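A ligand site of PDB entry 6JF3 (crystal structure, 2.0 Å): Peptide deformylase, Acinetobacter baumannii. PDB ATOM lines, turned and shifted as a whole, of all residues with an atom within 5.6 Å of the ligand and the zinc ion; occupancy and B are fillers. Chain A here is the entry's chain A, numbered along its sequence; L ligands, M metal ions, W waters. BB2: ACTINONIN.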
ATOM      1  N   ARG A  45      16.114  30.733 -19.822  1.00  0.00           N
ATOM      2  CA  ARG A  45      16.538  31.679 -20.867  1.00  0.00           C
ATOM      3  C   ARG A  45      16.640  31.007 -22.243  1.00  0.00           C
ATOM      4  O   ARG A  45      17.155  31.622 -23.192  1.00  0.00           O
ATOM      5  CB  ARG A  45      17.876  32.324 -20.525  1.00  0.00           C
ATOM      6  CG  ARG A  45      17.892  33.134 -19.218  1.00  0.00           C
ATOM      7  CD  ARG A  45      17.564  34.621 -19.371  1.00  0.00           C
ATOM      8  NE  ARG A  45      18.430  35.334 -20.338  1.00  0.00           N
ATOM      9  CZ  ARG A  45      18.858  36.602 -20.232  1.00  0.00           C
ATOM     10  NH1 ARG A  45      19.630  37.103 -21.197  1.00  0.00           N
ATOM     11  NH2 ARG A  45      18.529  37.370 -19.208  1.00  0.00           N
ATOM     12  N   ASN A  46      16.184  29.768 -22.377  1.00  0.00           N
ATOM     13  CA  ASN A  46      16.311  29.046 -23.661  1.00  0.00           C
ATOM     14  C   ASN A  46      17.726  28.990 -24.242  1.00  0.00           C
ATOM     15  O   ASN A  46      17.938  29.072 -25.450  1.00  0.00           O
ATOM     16  CB  ASN A  46      15.289  29.593 -24.673  1.00  0.00           C
ATOM     17  CG  ASN A  46      14.144  28.656 -24.858  1.00  0.00           C
ATOM     18  OD1 ASN A  46      14.251  27.684 -25.605  1.00  0.00           O
ATOM     19  ND2 ASN A  46      13.046  28.906 -24.160  1.00  0.00           N
ATOM     20  N   GLY A  47      18.716  28.844 -23.373  1.00  0.00           N
ATOM     21  CA  GLY A  47      20.090  28.629 -23.838  1.00  0.00           C
ATOM     22  C   GLY A  47      20.412  27.152 -23.969  1.00  0.00           C
ATOM     23  O   GLY A  47      19.698  26.294 -23.462  1.00  0.00           O
ATOM     24  N   VAL A  48      21.482  26.873 -24.691  1.00  0.00           N
ATOM     25  CA  VAL A  48      21.947  25.512 -24.907  1.00  0.00           C
ATOM     26  C   VAL A  48      23.250  25.275 -24.145  1.00  0.00           C
ATOM     27  O   VAL A  48      23.817  24.161 -24.223  1.00  0.00           O
ATOM     28  CB  VAL A  48      22.151  25.212 -26.397  1.00  0.00           C
ATOM     29  CG1 VAL A  48      20.809  25.163 -27.128  1.00  0.00           C
ATOM     30  CG2 VAL A  48      23.095  26.221 -27.042  1.00  0.00           C
ATOM     31  N   GLY A  49      23.726  26.340 -23.468  1.00  0.00           N
ATOM     32  CA  GLY A  49      24.734  26.236 -22.423  1.00  0.00           C
ATOM     33  C   GLY A  49      24.804  27.495 -21.549  1.00  0.00           C
ATOM     34  O   GLY A  49      24.099  28.516 -21.816  1.00  0.00           O
ATOM     35  N   ILE A  50      25.686  27.445 -20.550  1.00  0.00           N
ATOM     36  CA  ILE A  50      25.895  28.558 -19.611  1.00  0.00           C
ATOM     37  C   ILE A  50      27.220  28.445 -18.894  1.00  0.00           C
ATOM     38  O   ILE A  50      27.708  27.360 -18.674  1.00  0.00           O
ATOM     39  CB  ILE A  50      24.723  28.682 -18.603  1.00  0.00           C
ATOM     40  CG1 ILE A  50      24.761  30.013 -17.850  1.00  0.00           C
ATOM     41  CG2 ILE A  50      24.648  27.533 -17.626  1.00  0.00           C
ATOM     42  CD1 ILE A  50      23.367  30.435 -17.400  1.00  0.00           C
ATOM     43  N   ALA A  51      27.848  29.579 -18.591  1.00  0.00           N
ATOM     44  CA  ALA A  51      29.064  29.604 -17.813  1.00  0.00           C
ATOM     45  C   ALA A  51      28.830  30.432 -16.519  1.00  0.00           C
ATOM     46  O   ALA A  51      28.107  31.445 -16.496  1.00  0.00           O
ATOM     47  CB  ALA A  51      30.162  30.178 -18.673  1.00  0.00           C
ATOM     48  N   GLN A  54      28.473  34.316 -16.283  1.00  0.00           N
ATOM     49  CA  GLN A  54      27.262  34.910 -16.737  1.00  0.00           C
ATOM     50  C   GLN A  54      26.254  35.114 -15.645  1.00  0.00           C
ATOM     51  O   GLN A  54      25.410  35.969 -15.766  1.00  0.00           O
ATOM     52  CB  GLN A  54      26.633  34.053 -17.840  1.00  0.00           C
ATOM     53  CG  GLN A  54      27.452  33.998 -19.099  1.00  0.00           C
ATOM     54  CD  GLN A  54      26.810  33.187 -20.175  1.00  0.00           C
ATOM     55  OE1 GLN A  54      26.865  31.928 -20.128  1.00  0.00           O
ATOM     56  NE2 GLN A  54      26.205  33.869 -21.166  1.00  0.00           N
ATOM     57  N   ARG A  67      20.360  21.594 -27.441  1.00  0.00           N
ATOM     58  CA  ARG A  67      18.887  21.538 -27.409  1.00  0.00           C
ATOM     59  C   ARG A  67      18.287  21.049 -26.108  1.00  0.00           C
ATOM     60  O   ARG A  67      17.184  21.466 -25.756  1.00  0.00           O
ATOM     61  CB  ARG A  67      18.361  20.705 -28.553  1.00  0.00           C
ATOM     62  CG  ARG A  67      18.497  21.357 -29.900  1.00  0.00           C
ATOM     63  CD  ARG A  67      17.273  21.152 -30.753  1.00  0.00           C
ATOM     64  NE  ARG A  67      16.579  22.429 -30.861  1.00  0.00           N
ATOM     65  CZ  ARG A  67      15.694  22.921 -30.007  1.00  0.00           C
ATOM     66  NH1 ARG A  67      15.315  22.260 -28.915  1.00  0.00           N
ATOM     67  NH2 ARG A  67      15.157  24.116 -30.255  1.00  0.00           N
ATOM     68  N   ALA A  75      19.959  21.770 -34.166  1.00  0.00           N
ATOM     69  CA  ALA A  75      20.972  21.370 -33.160  1.00  0.00           C
ATOM     70  C   ALA A  75      20.742  19.937 -32.646  1.00  0.00           C
ATOM     71  O   ALA A  75      19.609  19.610 -32.260  1.00  0.00           O
ATOM     72  CB  ALA A  75      20.950  22.367 -32.008  1.00  0.00           C
ATOM     73  N   GLU A  99      25.846  30.488 -37.070  1.00  0.00           N
ATOM     74  CA  GLU A  99      25.362  31.621 -36.282  1.00  0.00           C
ATOM     75  C   GLU A  99      25.350  31.321 -34.754  1.00  0.00           C
ATOM     76  O   GLU A  99      24.750  30.328 -34.322  1.00  0.00           O
ATOM     77  CB  GLU A  99      23.983  32.108 -36.727  1.00  0.00           C
ATOM     78  CG  GLU A  99      23.561  33.379 -35.998  1.00  0.00           C
ATOM     79  CD  GLU A  99      22.364  34.050 -36.616  1.00  0.00           C
ATOM     80  OE1 GLU A  99      22.419  35.280 -36.803  1.00  0.00           O
ATOM     81  OE2 GLU A  99      21.374  33.349 -36.905  1.00  0.00           O
ATOM     82  N   GLU A 100      26.025  32.176 -33.964  1.00  0.00           N
ATOM     83  CA  GLU A 100      26.049  32.107 -32.479  1.00  0.00           C
ATOM     84  C   GLU A 100      25.378  33.361 -31.901  1.00  0.00           C
ATOM     85  O   GLU A 100      25.512  34.449 -32.430  1.00  0.00           O
ATOM     86  CB  GLU A 100      27.494  32.018 -31.912  1.00  0.00           C
ATOM     87  CG  GLU A 100      28.302  30.797 -32.379  1.00  0.00           C
ATOM     88  CD  GLU A 100      29.493  30.414 -31.479  1.00  0.00           C
ATOM     89  OE1 GLU A 100      29.831  31.118 -30.491  1.00  0.00           O
ATOM     90  OE2 GLU A 100      30.132  29.382 -31.760  1.00  0.00           O
ATOM     91  N   GLY A 101      24.646  33.171 -30.808  1.00  0.00           N
ATOM     92  CA  GLY A 101      24.169  34.262 -29.964  1.00  0.00           C
ATOM     93  C   GLY A 101      24.491  33.862 -28.544  1.00  0.00           C
ATOM     94  O   GLY A 101      24.844  32.736 -28.290  1.00  0.00           O
ATOM     95  N   CYS A 102      24.345  34.816 -27.631  1.00  0.00           N
ATOM     96  CA  CYS A 102      24.769  34.678 -26.246  1.00  0.00           C
ATOM     97  C   CYS A 102      23.691  35.321 -25.359  1.00  0.00           C
ATOM     98  O   CYS A 102      23.165  36.401 -25.686  1.00  0.00           O
ATOM     99  CB  CYS A 102      26.109  35.386 -26.099  1.00  0.00           C
ATOM    100  SG  CYS A 102      26.871  35.377 -24.470  1.00  0.00           S
ATOM    101  N   LEU A 103      23.357  34.639 -24.254  1.00  0.00           N
ATOM    102  CA  LEU A 103      22.404  35.176 -23.248  1.00  0.00           C
ATOM    103  C   LEU A 103      22.884  36.551 -22.703  1.00  0.00           C
ATOM    104  O   LEU A 103      22.056  37.319 -22.144  1.00  0.00           O
ATOM    105  CB  LEU A 103      22.209  34.230 -22.033  1.00  0.00           C
ATOM    106  CG  LEU A 103      21.749  32.776 -22.240  1.00  0.00           C
ATOM    107  CD1 LEU A 103      21.827  31.979 -20.924  1.00  0.00           C
ATOM    108  CD2 LEU A 103      20.356  32.721 -22.891  1.00  0.00           C
ATOM    109  N   SER A 104      24.196  36.812 -22.834  1.00  0.00           N
ATOM    110  CA  SER A 104      24.852  38.020 -22.339  1.00  0.00           C
ATOM    111  C   SER A 104      25.100  39.132 -23.396  1.00  0.00           C
ATOM    112  O   SER A 104      25.865  40.077 -23.100  1.00  0.00           O
ATOM    113  CB  SER A 104      26.199  37.619 -21.675  1.00  0.00           C
ATOM    114  OG  SER A 104      25.952  36.714 -20.601  1.00  0.00           O
ATOM    115  N   ARG A 109      24.101  38.795 -32.452  1.00  0.00           N
ATOM    116  CA  ARG A 109      24.441  37.525 -33.128  1.00  0.00           C
ATOM    117  C   ARG A 109      25.395  37.678 -34.350  1.00  0.00           C
ATOM    118  O   ARG A 109      25.764  38.795 -34.716  1.00  0.00           O
ATOM    119  CB  ARG A 109      23.152  36.754 -33.505  1.00  0.00           C
ATOM    120  CG  ARG A 109      22.035  36.915 -32.485  1.00  0.00           C
ATOM    121  CD  ARG A 109      21.226  35.634 -32.239  1.00  0.00           C
ATOM    122  NE  ARG A 109      20.564  35.108 -33.423  1.00  0.00           N
ATOM    123  CZ  ARG A 109      19.510  35.654 -34.042  1.00  0.00           C
ATOM    124  NH1 ARG A 109      18.976  35.050 -35.100  1.00  0.00           N
ATOM    125  NH2 ARG A 109      18.977  36.809 -33.621  1.00  0.00           N
ATOM    126  N   ARG A 114      34.580  27.869 -35.426  1.00  0.00           N
ATOM    127  CA  ARG A 114      34.978  27.029 -34.274  1.00  0.00           C
ATOM    128  C   ARG A 114      35.678  25.755 -34.731  1.00  0.00           C
ATOM    129  O   ARG A 114      35.413  25.268 -35.842  1.00  0.00           O
ATOM    130  CB  ARG A 114      33.730  26.628 -33.500  1.00  0.00           C
ATOM    131  CG  ARG A 114      32.926  27.755 -32.865  1.00  0.00           C
ATOM    132  CD  ARG A 114      33.730  28.438 -31.782  1.00  0.00           C
ATOM    133  NE  ARG A 114      32.892  29.351 -31.015  1.00  0.00           N
ATOM    134  CZ  ARG A 114      33.304  30.175 -30.069  1.00  0.00           C
ATOM    135  NH1 ARG A 114      34.576  30.241 -29.707  1.00  0.00           N
ATOM    136  NH2 ARG A 114      32.378  30.962 -29.497  1.00  0.00           N
ATOM    137  N   PHE A 137      28.027  20.924 -33.241  1.00  0.00           N
ATOM    138  CA  PHE A 137      27.453  21.981 -32.409  1.00  0.00           C
ATOM    139  C   PHE A 137      27.782  21.911 -30.909  1.00  0.00           C
ATOM    140  O   PHE A 137      28.222  22.894 -30.345  1.00  0.00           O
ATOM    141  CB  PHE A 137      25.958  22.084 -32.648  1.00  0.00           C
ATOM    142  CG  PHE A 137      25.344  23.336 -32.079  1.00  0.00           C
ATOM    143  CD1 PHE A 137      25.827  24.618 -32.432  1.00  0.00           C
ATOM    144  CD2 PHE A 137      24.233  23.259 -31.200  1.00  0.00           C
ATOM    145  CE1 PHE A 137      25.222  25.761 -31.933  1.00  0.00           C
ATOM    146  CE2 PHE A 137      23.635  24.407 -30.690  1.00  0.00           C
ATOM    147  CZ  PHE A 137      24.138  25.652 -31.051  1.00  0.00           C
ATOM    148  N   ARG A 140      31.077  23.425 -30.442  1.00  0.00           N
ATOM    149  CA  ARG A 140      30.981  24.879 -30.476  1.00  0.00           C
ATOM    150  C   ARG A 140      30.448  25.435 -29.138  1.00  0.00           C
ATOM    151  O   ARG A 140      30.956  26.427 -28.639  1.00  0.00           O
ATOM    152  CB  ARG A 140      30.098  25.375 -31.630  1.00  0.00           C
ATOM    153  CG  ARG A 140      30.726  25.130 -32.965  1.00  0.00           C
ATOM    154  N   ILE A 141      29.438  24.778 -28.561  1.00  0.00           N
ATOM    155  CA  ILE A 141      28.922  25.182 -27.299  1.00  0.00           C
ATOM    156  C   ILE A 141      30.048  25.144 -26.260  1.00  0.00           C
ATOM    157  O   ILE A 141      30.210  26.107 -25.551  1.00  0.00           O
ATOM    158  CB  ILE A 141      27.708  24.343 -26.793  1.00  0.00           C
ATOM    159  CG1 ILE A 141      26.523  24.416 -27.772  1.00  0.00           C
ATOM    160  CG2 ILE A 141      27.236  24.920 -25.468  1.00  0.00           C
ATOM    161  CD1 ILE A 141      25.430  23.379 -27.534  1.00  0.00           C
ATOM    162  N   HIS A 144      32.529  28.076 -26.809  1.00  0.00           N
ATOM    163  CA  HIS A 144      31.901  29.265 -26.349  1.00  0.00           C
ATOM    164  C   HIS A 144      31.892  29.443 -24.823  1.00  0.00           C
ATOM    165  O   HIS A 144      32.146  30.538 -24.324  1.00  0.00           O
ATOM    166  CB  HIS A 144      30.475  29.273 -26.879  1.00  0.00           C
ATOM    167  CG  HIS A 144      29.714  30.490 -26.548  1.00  0.00           C
ATOM    168  ND1 HIS A 144      29.465  31.480 -27.455  1.00  0.00           N
ATOM    169  CD2 HIS A 144      29.104  30.859 -25.397  1.00  0.00           C
ATOM    170  CE1 HIS A 144      28.724  32.416 -26.893  1.00  0.00           C
ATOM    171  NE2 HIS A 144      28.503  32.065 -25.645  1.00  0.00           N
ATOM    172  N   GLU A 145      31.551  28.384 -24.091  1.00  0.00           N
ATOM    173  CA  GLU A 145      31.442  28.505 -22.636  1.00  0.00           C
ATOM    174  C   GLU A 145      32.843  28.657 -22.002  1.00  0.00           C
ATOM    175  O   GLU A 145      33.054  29.506 -21.112  1.00  0.00           O
ATOM    176  CB  GLU A 145      30.718  27.294 -22.030  1.00  0.00           C
ATOM    177  CG  GLU A 145      29.297  27.029 -22.501  1.00  0.00           C
ATOM    178  CD  GLU A 145      28.419  28.232 -22.478  1.00  0.00           C
ATOM    179  OE1 GLU A 145      28.729  29.122 -21.643  1.00  0.00           O
ATOM    180  OE2 GLU A 145      27.421  28.282 -23.268  1.00  0.00           O
ATOM    181  N   HIS A 148      33.886  32.101 -22.240  1.00  0.00           N
ATOM    182  CA  HIS A 148      33.391  32.864 -21.141  1.00  0.00           C
ATOM    183  C   HIS A 148      34.282  32.786 -19.907  1.00  0.00           C
ATOM    184  O   HIS A 148      34.510  33.803 -19.271  1.00  0.00           O
ATOM    185  CB  HIS A 148      31.990  32.506 -20.763  1.00  0.00           C
ATOM    186  CG  HIS A 148      30.945  33.103 -21.629  1.00  0.00           C
ATOM    187  ND1 HIS A 148      30.751  34.468 -21.725  1.00  0.00           N
ATOM    188  CD2 HIS A 148      29.974  32.528 -22.379  1.00  0.00           C
ATOM    189  CE1 HIS A 148      29.718  34.710 -22.522  1.00  0.00           C
ATOM    190  NE2 HIS A 148      29.239  33.551 -22.957  1.00  0.00           N
HETATM  191  C5  BB2 L   1      23.977  30.700 -24.409  1.00  0.00           C
HETATM  192  C3  BB2 L   1      25.155  31.376 -23.754  1.00  0.00           C
HETATM  193  O4  BB2 L   1      25.310  32.578 -23.870  1.00  0.00           O
HETATM  194  N1  BB2 L   1      26.017  30.564 -23.119  1.00  0.00           N
HETATM  195  O2  BB2 L   1      27.239  31.029 -22.640  1.00  0.00           O
HETATM  196  C6  BB2 L   1      24.230  30.559 -25.913  1.00  0.00           C
HETATM  197  C12 BB2 L   1      22.910  30.215 -26.490  1.00  0.00           C
HETATM  198  O13 BB2 L   1      22.231  29.386 -25.919  1.00  0.00           O
HETATM  199  C7  BB2 L   1      25.233  29.450 -26.285  1.00  0.00           C
HETATM  200  C8  BB2 L   1      25.675  29.594 -27.757  1.00  0.00           C
HETATM  201  C9  BB2 L   1      26.552  28.457 -28.266  1.00  0.00           C
HETATM  202  C10 BB2 L   1      26.689  28.536 -29.780  1.00  0.00           C
HETATM  203  C11 BB2 L   1      27.868  27.728 -30.261  1.00  0.00           C
HETATM  204  N14 BB2 L   1      22.574  30.799 -27.644  1.00  0.00           N
HETATM  205  C15 BB2 L   1      21.381  30.370 -28.405  1.00  0.00           C
HETATM  206  C16 BB2 L   1      20.320  31.484 -28.352  1.00  0.00           C
HETATM  207  C18 BB2 L   1      20.039  31.873 -26.882  1.00  0.00           C
HETATM  208  C17 BB2 L   1      20.686  32.680 -29.226  1.00  0.00           C
HETATM  209  C19 BB2 L   1      21.782  29.857 -29.807  1.00  0.00           C
HETATM  210  O20 BB2 L   1      22.738  30.371 -30.408  1.00  0.00           O
HETATM  211  N21 BB2 L   1      21.067  28.795 -30.320  1.00  0.00           N
HETATM  212  C22 BB2 L   1      21.440  28.158 -31.603  1.00  0.00           C
HETATM  213  C23 BB2 L   1      19.886  28.129 -29.717  1.00  0.00           C
HETATM  214  C24 BB2 L   1      19.528  26.979 -30.642  1.00  0.00           C
HETATM  215  C25 BB2 L   1      20.685  26.828 -31.622  1.00  0.00           C
HETATM  216  C26 BB2 L   1      21.038  29.075 -32.773  1.00  0.00           C
HETATM  217  O27 BB2 L   1      22.191  29.707 -33.309  1.00  0.00           O
HETATM  218 ZN    ZN M   1      27.403  33.083 -24.091  1.00  0.00          ZN
HETATM  219  O   HOH W   1      29.625  35.028 -25.720  1.00  0.00           O
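N1 of the ligand lies within hydrogen-bond range of OE2 of Glu 145 (2.7 Å). N1 of the ligand is in hydrogen-bond range of OE1 of Gln 54, at 3.4 Å. An oxygen (O27) of the ligand is in hydrogen-bond range of the backbone carbonyl oxygen (O) of Glu 99 (2.8 Å). An oxygen (O4) of the ligand sits close to the backbone NH (N) of Leu 103, 2.9 Å away. The backbone NH of Val 48 is in hydrogen-bond range of an oxygen (O13) of the ligand. The backbone NH (N) of Gly 101 is in hydrogen-bond range of an oxygen (O20) of the ligand, at 3.4 Å. The backbone carbonyl oxygen (O) of Gly 101 is in hydrogen-bond range of a nitrogen (N14) of the ligand (3.1 Å). The backbone carbonyl oxygen (O) of Gly 49 sits at hydrogen-bond distance from a nitrogen (N1) of the ligand, 3.1 Å away.
SG of Cys 102 sits close to NE2 of Gln 54 (3.7 Å). The side-chain sulfur (SG) of Cys 102 lies close to the backbone NH (N) of Ser 104 (3.4 Å). The backbone NH (N) of Ile 50 sits at hydrogen-bond distance from the side-chain carboxylate (OE2) of Glu 145 (3.3 Å). The backbone NH (N) of Ala 51 is in hydrogen-bond range of the side-chain carboxylate (OE1) of Glu 145, 3.2 Å away. The backbone NH of Ala 51 lies within hydrogen-bond range of the side-chain amide oxygen of Gln 54 (3.0 Å). The side-chain carboxylate (OE2) of Glu 99 lies within salt-bridge range of the guanidinium group (NH1) of Arg 109 (3.4 Å). O of Leu 103 lies within hydrogen-bond range of NH1 of Arg 45 (2.6 Å). The side-chain carboxylate (OE1) of Glu 100 is in salt-bridge range of the guanidinium group (NH2) of Arg 114, at 2.7 Å.
Residues that only touch the ligand: Gly 47 (3.1 Å), Glu 100 (3.2 Å), Arg 140 (3.5 Å), Phe 137 (3.7 Å), Ile 141 (3.7 Å) and Asn 46 (3.8 Å). Hydrophobic or aromatic side chains within 4 Å of the ligand: Val 48, Leu 103, Phe 137, His 144 and His 148. Of the 24 residues printed, 16 come within 4 Å of the ligand. The nearest printed residue that does not touch the ligand is Ile 50 (4.04 Å).
NE2 of Gln 54 touches the zinc ion, 3.3 Å away. Within 4 Å of the zinc ion: Gln 54, Cys 102, His 144 and His 148. The nearest printed residue that does not touch the zinc ion is Leu 103 (4.3 Å).
A ring nitrogen (NE2) of His 144 is bound to the zinc ion, at 2.2 Å. The zinc ion is bound by an oxygen (O4) of the ligand, at 2.2 Å. The zinc ion is bound by NE2 of His 148 (2.2 Å). The zinc ion is bound by SG of Cys 102, 2.4 Å away. O2 of the ligand is bound to the zinc ion, 2.5 Å away. The zinc ion has five donor atoms within binding distance.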
